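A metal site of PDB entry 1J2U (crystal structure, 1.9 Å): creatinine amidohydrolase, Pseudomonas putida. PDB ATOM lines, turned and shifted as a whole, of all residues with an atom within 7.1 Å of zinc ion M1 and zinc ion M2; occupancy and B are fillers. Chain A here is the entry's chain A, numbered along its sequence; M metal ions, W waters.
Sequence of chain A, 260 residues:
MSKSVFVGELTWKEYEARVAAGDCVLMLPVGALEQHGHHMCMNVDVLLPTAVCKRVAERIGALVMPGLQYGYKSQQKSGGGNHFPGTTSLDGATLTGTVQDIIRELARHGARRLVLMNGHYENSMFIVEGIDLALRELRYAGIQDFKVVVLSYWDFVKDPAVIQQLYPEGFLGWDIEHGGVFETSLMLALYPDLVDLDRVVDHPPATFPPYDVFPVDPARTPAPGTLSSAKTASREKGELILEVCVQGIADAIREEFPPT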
ATOM      1  N   GLY A  31      31.338  -0.894 -17.788  1.00  0.00           N
ATOM      2  CA  GLY A  31      31.145  -0.057 -16.632  1.00  0.00           C
ATOM      3  C   GLY A  31      29.946   0.871 -16.623  1.00  0.00           C
ATOM      4  O   GLY A  31      28.852   0.509 -17.033  1.00  0.00           O
ATOM      5  N   ALA A  32      30.160   2.066 -16.088  1.00  0.00           N
ATOM      6  CA  ALA A  32      29.121   3.075 -15.926  1.00  0.00           C
ATOM      7  C   ALA A  32      29.739   4.364 -15.452  1.00  0.00           C
ATOM      8  O   ALA A  32      30.886   4.405 -14.977  1.00  0.00           O
ATOM      9  CB  ALA A  32      28.071   2.611 -14.886  1.00  0.00           C
ATOM     10  N   LEU A  33      28.970   5.439 -15.618  1.00  0.00           N
ATOM     11  CA  LEU A  33      29.287   6.745 -15.070  1.00  0.00           C
ATOM     12  C   LEU A  33      28.161   6.958 -14.049  1.00  0.00           C
ATOM     13  O   LEU A  33      26.986   7.135 -14.415  1.00  0.00           O
ATOM     14  CB  LEU A  33      29.308   7.838 -16.145  1.00  0.00           C
ATOM     15  CG  LEU A  33      29.614   9.251 -15.608  1.00  0.00           C
ATOM     16  CD1 LEU A  33      31.036   9.347 -15.055  1.00  0.00           C
ATOM     17  CD2 LEU A  33      29.385  10.349 -16.683  1.00  0.00           C
ATOM     18  N   GLU A  34      28.513   6.883 -12.758  1.00  0.00           N
ATOM     19  CA  GLU A  34      27.533   6.806 -11.694  1.00  0.00           C
ATOM     20  C   GLU A  34      28.071   7.438 -10.413  1.00  0.00           C
ATOM     21  O   GLU A  34      29.219   7.263 -10.060  1.00  0.00           O
ATOM     22  CB  GLU A  34      27.144   5.340 -11.447  1.00  0.00           C
ATOM     23  CG  GLU A  34      26.163   5.070 -10.296  1.00  0.00           C
ATOM     24  CD  GLU A  34      25.913   3.575 -10.051  1.00  0.00           C
ATOM     25  OE1 GLU A  34      24.750   3.126  -9.915  1.00  0.00           O
ATOM     26  OE2 GLU A  34      26.910   2.844 -10.000  1.00  0.00           O
ATOM     27  N   GLN A  35      27.229   8.193  -9.740  1.00  0.00           N
ATOM     28  CA  GLN A  35      27.591   8.786  -8.466  1.00  0.00           C
ATOM     29  C   GLN A  35      28.121   7.693  -7.559  1.00  0.00           C
ATOM     30  O   GLN A  35      27.589   6.589  -7.544  1.00  0.00           O
ATOM     31  CB  GLN A  35      26.375   9.416  -7.817  1.00  0.00           C
ATOM     32  CG  GLN A  35      25.255   8.455  -7.408  1.00  0.00           C
ATOM     33  CD  GLN A  35      25.431   7.894  -6.003  1.00  0.00           C
ATOM     34  OE1 GLN A  35      26.228   8.409  -5.227  1.00  0.00           O
ATOM     35  NE2 GLN A  35      24.663   6.839  -5.677  1.00  0.00           N
ATOM     36  N   HIS A  36      29.166   8.001  -6.806  1.00  0.00           N
ATOM     37  CA  HIS A  36      29.710   7.091  -5.812  1.00  0.00           C
ATOM     38  C   HIS A  36      29.962   7.849  -4.495  1.00  0.00           C
ATOM     39  O   HIS A  36      31.064   7.800  -3.967  1.00  0.00           O
ATOM     40  CB  HIS A  36      30.983   6.447  -6.292  1.00  0.00           C
ATOM     41  CG  HIS A  36      30.766   5.243  -7.151  1.00  0.00           C
ATOM     42  ND1 HIS A  36      30.345   5.323  -8.461  1.00  0.00           N
ATOM     43  CD2 HIS A  36      30.903   3.921  -6.886  1.00  0.00           C
ATOM     44  CE1 HIS A  36      30.225   4.107  -8.963  1.00  0.00           C
ATOM     45  NE2 HIS A  36      30.557   3.238  -8.018  1.00  0.00           N
ATOM     46  N   MET A  40      34.316   9.774  -3.517  1.00  0.00           N
ATOM     47  CA  MET A  40      34.913   9.074  -4.647  1.00  0.00           C
ATOM     48  C   MET A  40      34.350   9.613  -5.945  1.00  0.00           C
ATOM     49  O   MET A  40      33.235  10.109  -5.978  1.00  0.00           O
ATOM     50  CB  MET A  40      34.547   7.587  -4.548  1.00  0.00           C
ATOM     51  CG  MET A  40      35.565   6.658  -5.104  1.00  0.00           C
ATOM     52  SD  MET A  40      35.518   5.045  -4.339  1.00  0.00           S
ATOM     53  CE  MET A  40      33.790   4.745  -4.162  1.00  0.00           C
ATOM     54  N   MET A  42      33.135   9.466 -10.158  1.00  0.00           N
ATOM     55  CA  MET A  42      32.027   8.771 -10.823  1.00  0.00           C
ATOM     56  C   MET A  42      32.356   7.700 -11.872  1.00  0.00           C
ATOM     57  O   MET A  42      31.453   6.979 -12.319  1.00  0.00           O
ATOM     58  CB  MET A  42      31.057   9.815 -11.405  1.00  0.00           C
ATOM     59  CG  MET A  42      30.393  10.662 -10.315  1.00  0.00           C
ATOM     60  SD  MET A  42      29.107  11.749 -10.967  1.00  0.00           S
ATOM     61  CE  MET A  42      30.074  12.937 -11.798  1.00  0.00           C
ATOM     62  N   VAL A  44      34.364   5.087 -11.322  1.00  0.00           N
ATOM     63  CA  VAL A  44      34.831   3.877 -10.624  1.00  0.00           C
ATOM     64  C   VAL A  44      34.504   2.561 -11.324  1.00  0.00           C
ATOM     65  O   VAL A  44      35.333   1.661 -11.389  1.00  0.00           O
ATOM     66  CB  VAL A  44      34.253   3.871  -9.175  1.00  0.00           C
ATOM     67  CG1 VAL A  44      34.365   2.513  -8.506  1.00  0.00           C
ATOM     68  CG2 VAL A  44      34.928   4.961  -8.344  1.00  0.00           C
ATOM     69  N   ASP A  45      33.288   2.432 -11.830  1.00  0.00           N
ATOM     70  CA  ASP A  45      32.812   1.182 -12.432  1.00  0.00           C
ATOM     71  C   ASP A  45      33.465   0.868 -13.762  1.00  0.00           C
ATOM     72  O   ASP A  45      33.356  -0.269 -14.230  1.00  0.00           O
ATOM     73  CB  ASP A  45      31.302   1.171 -12.558  1.00  0.00           C
ATOM     74  CG  ASP A  45      30.607   1.156 -11.213  1.00  0.00           C
ATOM     75  OD1 ASP A  45      31.264   1.052 -10.146  1.00  0.00           O
ATOM     76  OD2 ASP A  45      29.377   1.250 -11.154  1.00  0.00           O
ATOM     77  N   VAL A  46      34.111   1.865 -14.361  1.00  0.00           N
ATOM     78  CA  VAL A  46      34.987   1.633 -15.521  1.00  0.00           C
ATOM     79  C   VAL A  46      36.424   1.350 -15.043  1.00  0.00           C
ATOM     80  O   VAL A  46      37.056   0.380 -15.469  1.00  0.00           O
ATOM     81  CB  VAL A  46      35.041   2.837 -16.491  1.00  0.00           C
ATOM     82  CG1 VAL A  46      36.028   2.545 -17.612  1.00  0.00           C
ATOM     83  CG2 VAL A  46      33.660   3.165 -17.037  1.00  0.00           C
ATOM     84  N   LEU A  48      37.792   0.264 -12.208  1.00  0.00           N
ATOM     85  CA  LEU A  48      38.052  -0.963 -11.472  1.00  0.00           C
ATOM     86  C   LEU A  48      38.101  -2.240 -12.343  1.00  0.00           C
ATOM     87  O   LEU A  48      39.117  -2.928 -12.355  1.00  0.00           O
ATOM     88  CB  LEU A  48      37.071  -1.061 -10.305  1.00  0.00           C
ATOM     89  CG  LEU A  48      37.295   0.029  -9.254  1.00  0.00           C
ATOM     90  CD1 LEU A  48      36.495  -0.247  -8.009  1.00  0.00           C
ATOM     91  CD2 LEU A  48      38.763   0.236  -8.867  1.00  0.00           C
ATOM     92  N   TYR A  72      23.699   0.665 -17.664  1.00  0.00           N
ATOM     93  CA  TYR A  72      22.279   0.681 -17.409  1.00  0.00           C
ATOM     94  C   TYR A  72      21.938   1.600 -16.216  1.00  0.00           C
ATOM     95  O   TYR A  72      22.794   1.832 -15.327  1.00  0.00           O
ATOM     96  CB  TYR A  72      21.662  -0.724 -17.245  1.00  0.00           C
ATOM     97  CG  TYR A  72      20.173  -0.630 -17.176  1.00  0.00           C
ATOM     98  CD1 TYR A  72      19.438  -0.177 -18.263  1.00  0.00           C
ATOM     99  CD2 TYR A  72      19.481  -0.908 -16.000  1.00  0.00           C
ATOM    100  CE1 TYR A  72      18.068  -0.039 -18.194  1.00  0.00           C
ATOM    101  CE2 TYR A  72      18.124  -0.755 -15.910  1.00  0.00           C
ATOM    102  CZ  TYR A  72      17.411  -0.312 -17.004  1.00  0.00           C
ATOM    103  OH  TYR A  72      16.052  -0.158 -16.895  1.00  0.00           O
ATOM    104  N   SER A  74      21.037   3.296 -12.925  1.00  0.00           N
ATOM    105  CA  SER A  74      21.259   2.994 -11.518  1.00  0.00           C
ATOM    106  C   SER A  74      19.928   2.685 -10.808  1.00  0.00           C
ATOM    107  O   SER A  74      18.942   3.442 -10.971  1.00  0.00           O
ATOM    108  CB  SER A  74      21.932   4.205 -10.869  1.00  0.00           C
ATOM    109  OG  SER A  74      22.112   4.035  -9.478  1.00  0.00           O
ATOM    110  N   SER A  78      20.695  -0.922  -5.393  1.00  0.00           N
ATOM    111  CA  SER A  78      22.046  -1.337  -5.753  1.00  0.00           C
ATOM    112  C   SER A  78      23.029  -0.210  -6.142  1.00  0.00           C
ATOM    113  O   SER A  78      24.243  -0.441  -6.241  1.00  0.00           O
ATOM    114  CB  SER A  78      21.992  -2.346  -6.903  1.00  0.00           C
ATOM    115  OG  SER A  78      21.224  -1.868  -7.986  1.00  0.00           O
ATOM    116  N   GLY A  79      22.509   1.007  -6.352  1.00  0.00           N
ATOM    117  CA  GLY A  79      23.330   2.142  -6.760  1.00  0.00           C
ATOM    118  C   GLY A  79      22.799   3.513  -6.369  1.00  0.00           C
ATOM    119  O   GLY A  79      23.284   4.529  -6.867  1.00  0.00           O
ATOM    120  N   GLY A 119      31.458  -4.223 -14.233  1.00  0.00           N
ATOM    121  CA  GLY A 119      31.830  -3.446 -13.066  1.00  0.00           C
ATOM    122  C   GLY A 119      30.722  -2.631 -12.450  1.00  0.00           C
ATOM    123  O   GLY A 119      30.954  -1.959 -11.441  1.00  0.00           O
ATOM    124  N   HIS A 120      29.516  -2.737 -13.017  1.00  0.00           N
ATOM    125  CA  HIS A 120      28.328  -1.956 -12.590  1.00  0.00           C
ATOM    126  C   HIS A 120      27.192  -2.933 -12.404  1.00  0.00           C
ATOM    127  O   HIS A 120      26.790  -3.638 -13.339  1.00  0.00           O
ATOM    128  CB  HIS A 120      28.038  -0.910 -13.677  1.00  0.00           C
ATOM    129  CG  HIS A 120      26.773  -0.132 -13.491  1.00  0.00           C
ATOM    130  ND1 HIS A 120      26.549   0.716 -12.420  1.00  0.00           N
ATOM    131  CD2 HIS A 120      25.691  -0.013 -14.297  1.00  0.00           C
ATOM    132  CE1 HIS A 120      25.373   1.309 -12.571  1.00  0.00           C
ATOM    133  NE2 HIS A 120      24.831   0.881 -13.709  1.00  0.00           N
ATOM    134  N   TYR A 121      26.701  -3.001 -11.183  1.00  0.00           N
ATOM    135  CA  TYR A 121      25.760  -4.037 -10.767  1.00  0.00           C
ATOM    136  C   TYR A 121      24.563  -4.214 -11.691  1.00  0.00           C
ATOM    137  O   TYR A 121      24.211  -5.345 -12.046  1.00  0.00           O
ATOM    138  CB  TYR A 121      25.275  -3.728  -9.355  1.00  0.00           C
ATOM    139  CG  TYR A 121      24.583  -4.863  -8.669  1.00  0.00           C
ATOM    140  CD1 TYR A 121      25.290  -5.741  -7.861  1.00  0.00           C
ATOM    141  CD2 TYR A 121      23.222  -5.087  -8.840  1.00  0.00           C
ATOM    142  CE1 TYR A 121      24.670  -6.788  -7.224  1.00  0.00           C
ATOM    143  CE2 TYR A 121      22.590  -6.134  -8.224  1.00  0.00           C
ATOM    144  CZ  TYR A 121      23.326  -6.985  -7.395  1.00  0.00           C
ATOM    145  OH  TYR A 121      22.737  -8.056  -6.742  1.00  0.00           O
ATOM    146  N   GLU A 122      23.992  -3.096 -12.140  1.00  0.00           N
ATOM    147  CA  GLU A 122      22.801  -3.095 -12.968  1.00  0.00           C
ATOM    148  C   GLU A 122      22.946  -3.508 -14.441  1.00  0.00           C
ATOM    149  O   GLU A 122      21.920  -3.734 -15.107  1.00  0.00           O
ATOM    150  CB  GLU A 122      22.197  -1.665 -12.924  1.00  0.00           C
ATOM    151  CG  GLU A 122      21.632  -1.286 -11.558  1.00  0.00           C
ATOM    152  CD  GLU A 122      22.624  -0.622 -10.621  1.00  0.00           C
ATOM    153  OE1 GLU A 122      23.848  -0.666 -10.877  1.00  0.00           O
ATOM    154  OE2 GLU A 122      22.161  -0.032  -9.616  1.00  0.00           O
ATOM    155  N   TYR A 153      33.302  -8.848 -11.391  1.00  0.00           N
ATOM    156  CA  TYR A 153      34.594  -9.167 -10.756  1.00  0.00           C
ATOM    157  C   TYR A 153      34.502  -9.406  -9.250  1.00  0.00           C
ATOM    158  O   TYR A 153      35.239 -10.258  -8.723  1.00  0.00           O
ATOM    159  CB  TYR A 153      35.684  -8.156 -11.122  1.00  0.00           C
ATOM    160  CG  TYR A 153      35.510  -6.826 -10.472  1.00  0.00           C
ATOM    161  CD1 TYR A 153      36.109  -6.534  -9.265  1.00  0.00           C
ATOM    162  CD2 TYR A 153      34.706  -5.857 -11.057  1.00  0.00           C
ATOM    163  CE1 TYR A 153      35.927  -5.319  -8.636  1.00  0.00           C
ATOM    164  CE2 TYR A 153      34.512  -4.626 -10.441  1.00  0.00           C
ATOM    165  CZ  TYR A 153      35.114  -4.371  -9.231  1.00  0.00           C
ATOM    166  OH  TYR A 153      34.939  -3.163  -8.611  1.00  0.00           O
ATOM    167  N   TRP A 154      33.612  -8.687  -8.569  1.00  0.00           N
ATOM    168  CA  TRP A 154      33.440  -8.873  -7.127  1.00  0.00           C
ATOM    169  C   TRP A 154      32.943 -10.249  -6.700  1.00  0.00           C
ATOM    170  O   TRP A 154      33.217 -10.677  -5.568  1.00  0.00           O
ATOM    171  CB  TRP A 154      32.496  -7.829  -6.553  1.00  0.00           C
ATOM    172  CG  TRP A 154      31.160  -7.771  -7.211  1.00  0.00           C
ATOM    173  CD1 TRP A 154      30.063  -8.561  -6.967  1.00  0.00           C
ATOM    174  CD2 TRP A 154      30.756  -6.842  -8.221  1.00  0.00           C
ATOM    175  NE1 TRP A 154      29.006  -8.158  -7.754  1.00  0.00           N
ATOM    176  CE2 TRP A 154      29.410  -7.122  -8.556  1.00  0.00           C
ATOM    177  CE3 TRP A 154      31.393  -5.798  -8.885  1.00  0.00           C
ATOM    178  CZ2 TRP A 154      28.700  -6.391  -9.514  1.00  0.00           C
ATOM    179  CZ3 TRP A 154      30.697  -5.084  -9.849  1.00  0.00           C
ATOM    180  CH2 TRP A 154      29.365  -5.383 -10.141  1.00  0.00           C
ATOM    181  N   GLU A 177      26.631  -2.993  -1.447  1.00  0.00           N
ATOM    182  CA  GLU A 177      27.995  -2.533  -1.631  1.00  0.00           C
ATOM    183  C   GLU A 177      28.002  -1.591  -2.825  1.00  0.00           C
ATOM    184  O   GLU A 177      28.262  -2.020  -3.970  1.00  0.00           O
ATOM    185  CB  GLU A 177      28.973  -3.663  -1.971  1.00  0.00           C
ATOM    186  CG  GLU A 177      29.784  -4.212  -0.826  1.00  0.00           C
ATOM    187  CD  GLU A 177      30.449  -3.143   0.007  1.00  0.00           C
ATOM    188  OE1 GLU A 177      30.113  -3.081   1.185  1.00  0.00           O
ATOM    189  OE2 GLU A 177      31.293  -2.375  -0.518  1.00  0.00           O
ATOM    190  N   HIS A 178      27.657  -0.344  -2.583  1.00  0.00           N
ATOM    191  CA  HIS A 178      27.827   0.673  -3.593  1.00  0.00           C
ATOM    192  C   HIS A 178      28.515   1.816  -2.886  1.00  0.00           C
ATOM    193  O   HIS A 178      27.950   2.410  -1.974  1.00  0.00           O
ATOM    194  CB  HIS A 178      26.508   1.149  -4.175  1.00  0.00           C
ATOM    195  CG  HIS A 178      26.650   2.351  -5.044  1.00  0.00           C
ATOM    196  ND1 HIS A 178      27.329   2.329  -6.245  1.00  0.00           N
ATOM    197  CD2 HIS A 178      26.202   3.617  -4.885  1.00  0.00           C
ATOM    198  CE1 HIS A 178      27.308   3.539  -6.780  1.00  0.00           C
ATOM    199  NE2 HIS A 178      26.625   4.329  -5.980  1.00  0.00           N
ATOM    200  N   GLY A 179      29.741   2.094  -3.302  1.00  0.00           N
ATOM    201  CA  GLY A 179      30.535   3.164  -2.748  1.00  0.00           C
ATOM    202  C   GLY A 179      31.047   2.887  -1.349  1.00  0.00           C
ATOM    203  O   GLY A 179      31.466   3.822  -0.655  1.00  0.00           O
ATOM    204  N   GLU A 183      34.705  -1.103  -2.959  1.00  0.00           N
ATOM    205  CA  GLU A 183      35.183  -0.237  -4.030  1.00  0.00           C
ATOM    206  C   GLU A 183      36.170   0.806  -3.552  1.00  0.00           C
ATOM    207  O   GLU A 183      37.139   1.113  -4.234  1.00  0.00           O
ATOM    208  CB  GLU A 183      33.999   0.458  -4.717  1.00  0.00           C
ATOM    209  CG  GLU A 183      33.148  -0.481  -5.512  1.00  0.00           C
ATOM    210  CD  GLU A 183      32.048   0.258  -6.263  1.00  0.00           C
ATOM    211  OE1 GLU A 183      31.985   0.087  -7.479  1.00  0.00           O
ATOM    212  OE2 GLU A 183      31.266   0.990  -5.622  1.00  0.00           O
HETATM  213 ZN    ZN M   1      27.528   0.969 -10.336  1.00  0.00          ZN
HETATM  214 ZN    ZN M   2      30.534   1.227  -8.317  1.00  0.00          ZN
HETATM  215  O   HOH W   1      29.746  -1.743  -8.914  1.00  0.00           O
HETATM  216  O   HOH W   2      27.334  -0.637  -9.600  1.00  0.00           O
HETATM  217  O   HOH W   3      25.409   0.463  -8.924  1.00  0.00           O
HETATM  218  O   HOH W   4      28.923   0.586  -7.965  1.00  0.00           O
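N of Gly 179 lies within hydrogen-bond range of OE2 of Glu 183 (3.0 Å).
OE1 of Glu 122 sits close to NE2 of His 120 (3.4 Å).
NE2 of His 178 lies within hydrogen-bond range of O of Gly 79.
NE2 of His 120 sits at hydrogen-bond distance from O of Tyr 72 (2.8 Å).
A ring nitrogen (NE2) of His 178 lies within hydrogen-bond range of the backbone carbonyl oxygen (O) of Gln 35, 2.9 Å away.
The side-chain carboxylate (OE1) of Glu 34 is in hydrogen-bond range of the side-chain hydroxyl (OG) of Ser 74 (2.8 Å).
O of Glu 34 sits at hydrogen-bond distance from ND1 of His 36, at 2.8 Å.
N of Glu 34 sits at hydrogen-bond distance from O of Met 42.
Three residues have an atom within 4 Å of zinc ion M1: Glu 34, Asp 45 and His 120.
His 178 touches zinc ion M2 (ND1 to ZN, 3.97 Å).
Within 4 Å of zinc ion M2: His 36, Asp 45, His 178 and Glu 183.
Water W2 binds zinc ion M1, at 1.8 Å.
OE2 of Glu 34 is bound to zinc ion M1, 2.0 Å away.
The side-chain carboxylate (OD2) of Asp 45 binds zinc ion M1, 2.0 Å away.
ND1 of His 120 is bound to zinc ion M1 (2.3 Å).
Water W3 binds zinc ion M1 (2.6 Å).
Zinc ion M1 has five donor atoms within binding distance.
Slightly farther from zinc ion M1 lies water W4 (2.8 Å).
Zinc ion M2 is bound by water W4 (1.8 Å), the side-chain carboxylate (OD1) of Asp 45 (2.0 Å), the side-chain carboxylate (OE1) of Glu 183 (2.0 Å) and a ring nitrogen (NE2) of His 36 (2.0 Å).
Slightly farther from zinc ion M2 lies OE2 of Glu 183 (2.8 Å).
Water W4 lies within hydrogen-bond range of a ring nitrogen (ND1) of His 178 and the side-chain carboxylate (OE2) of Glu 183.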
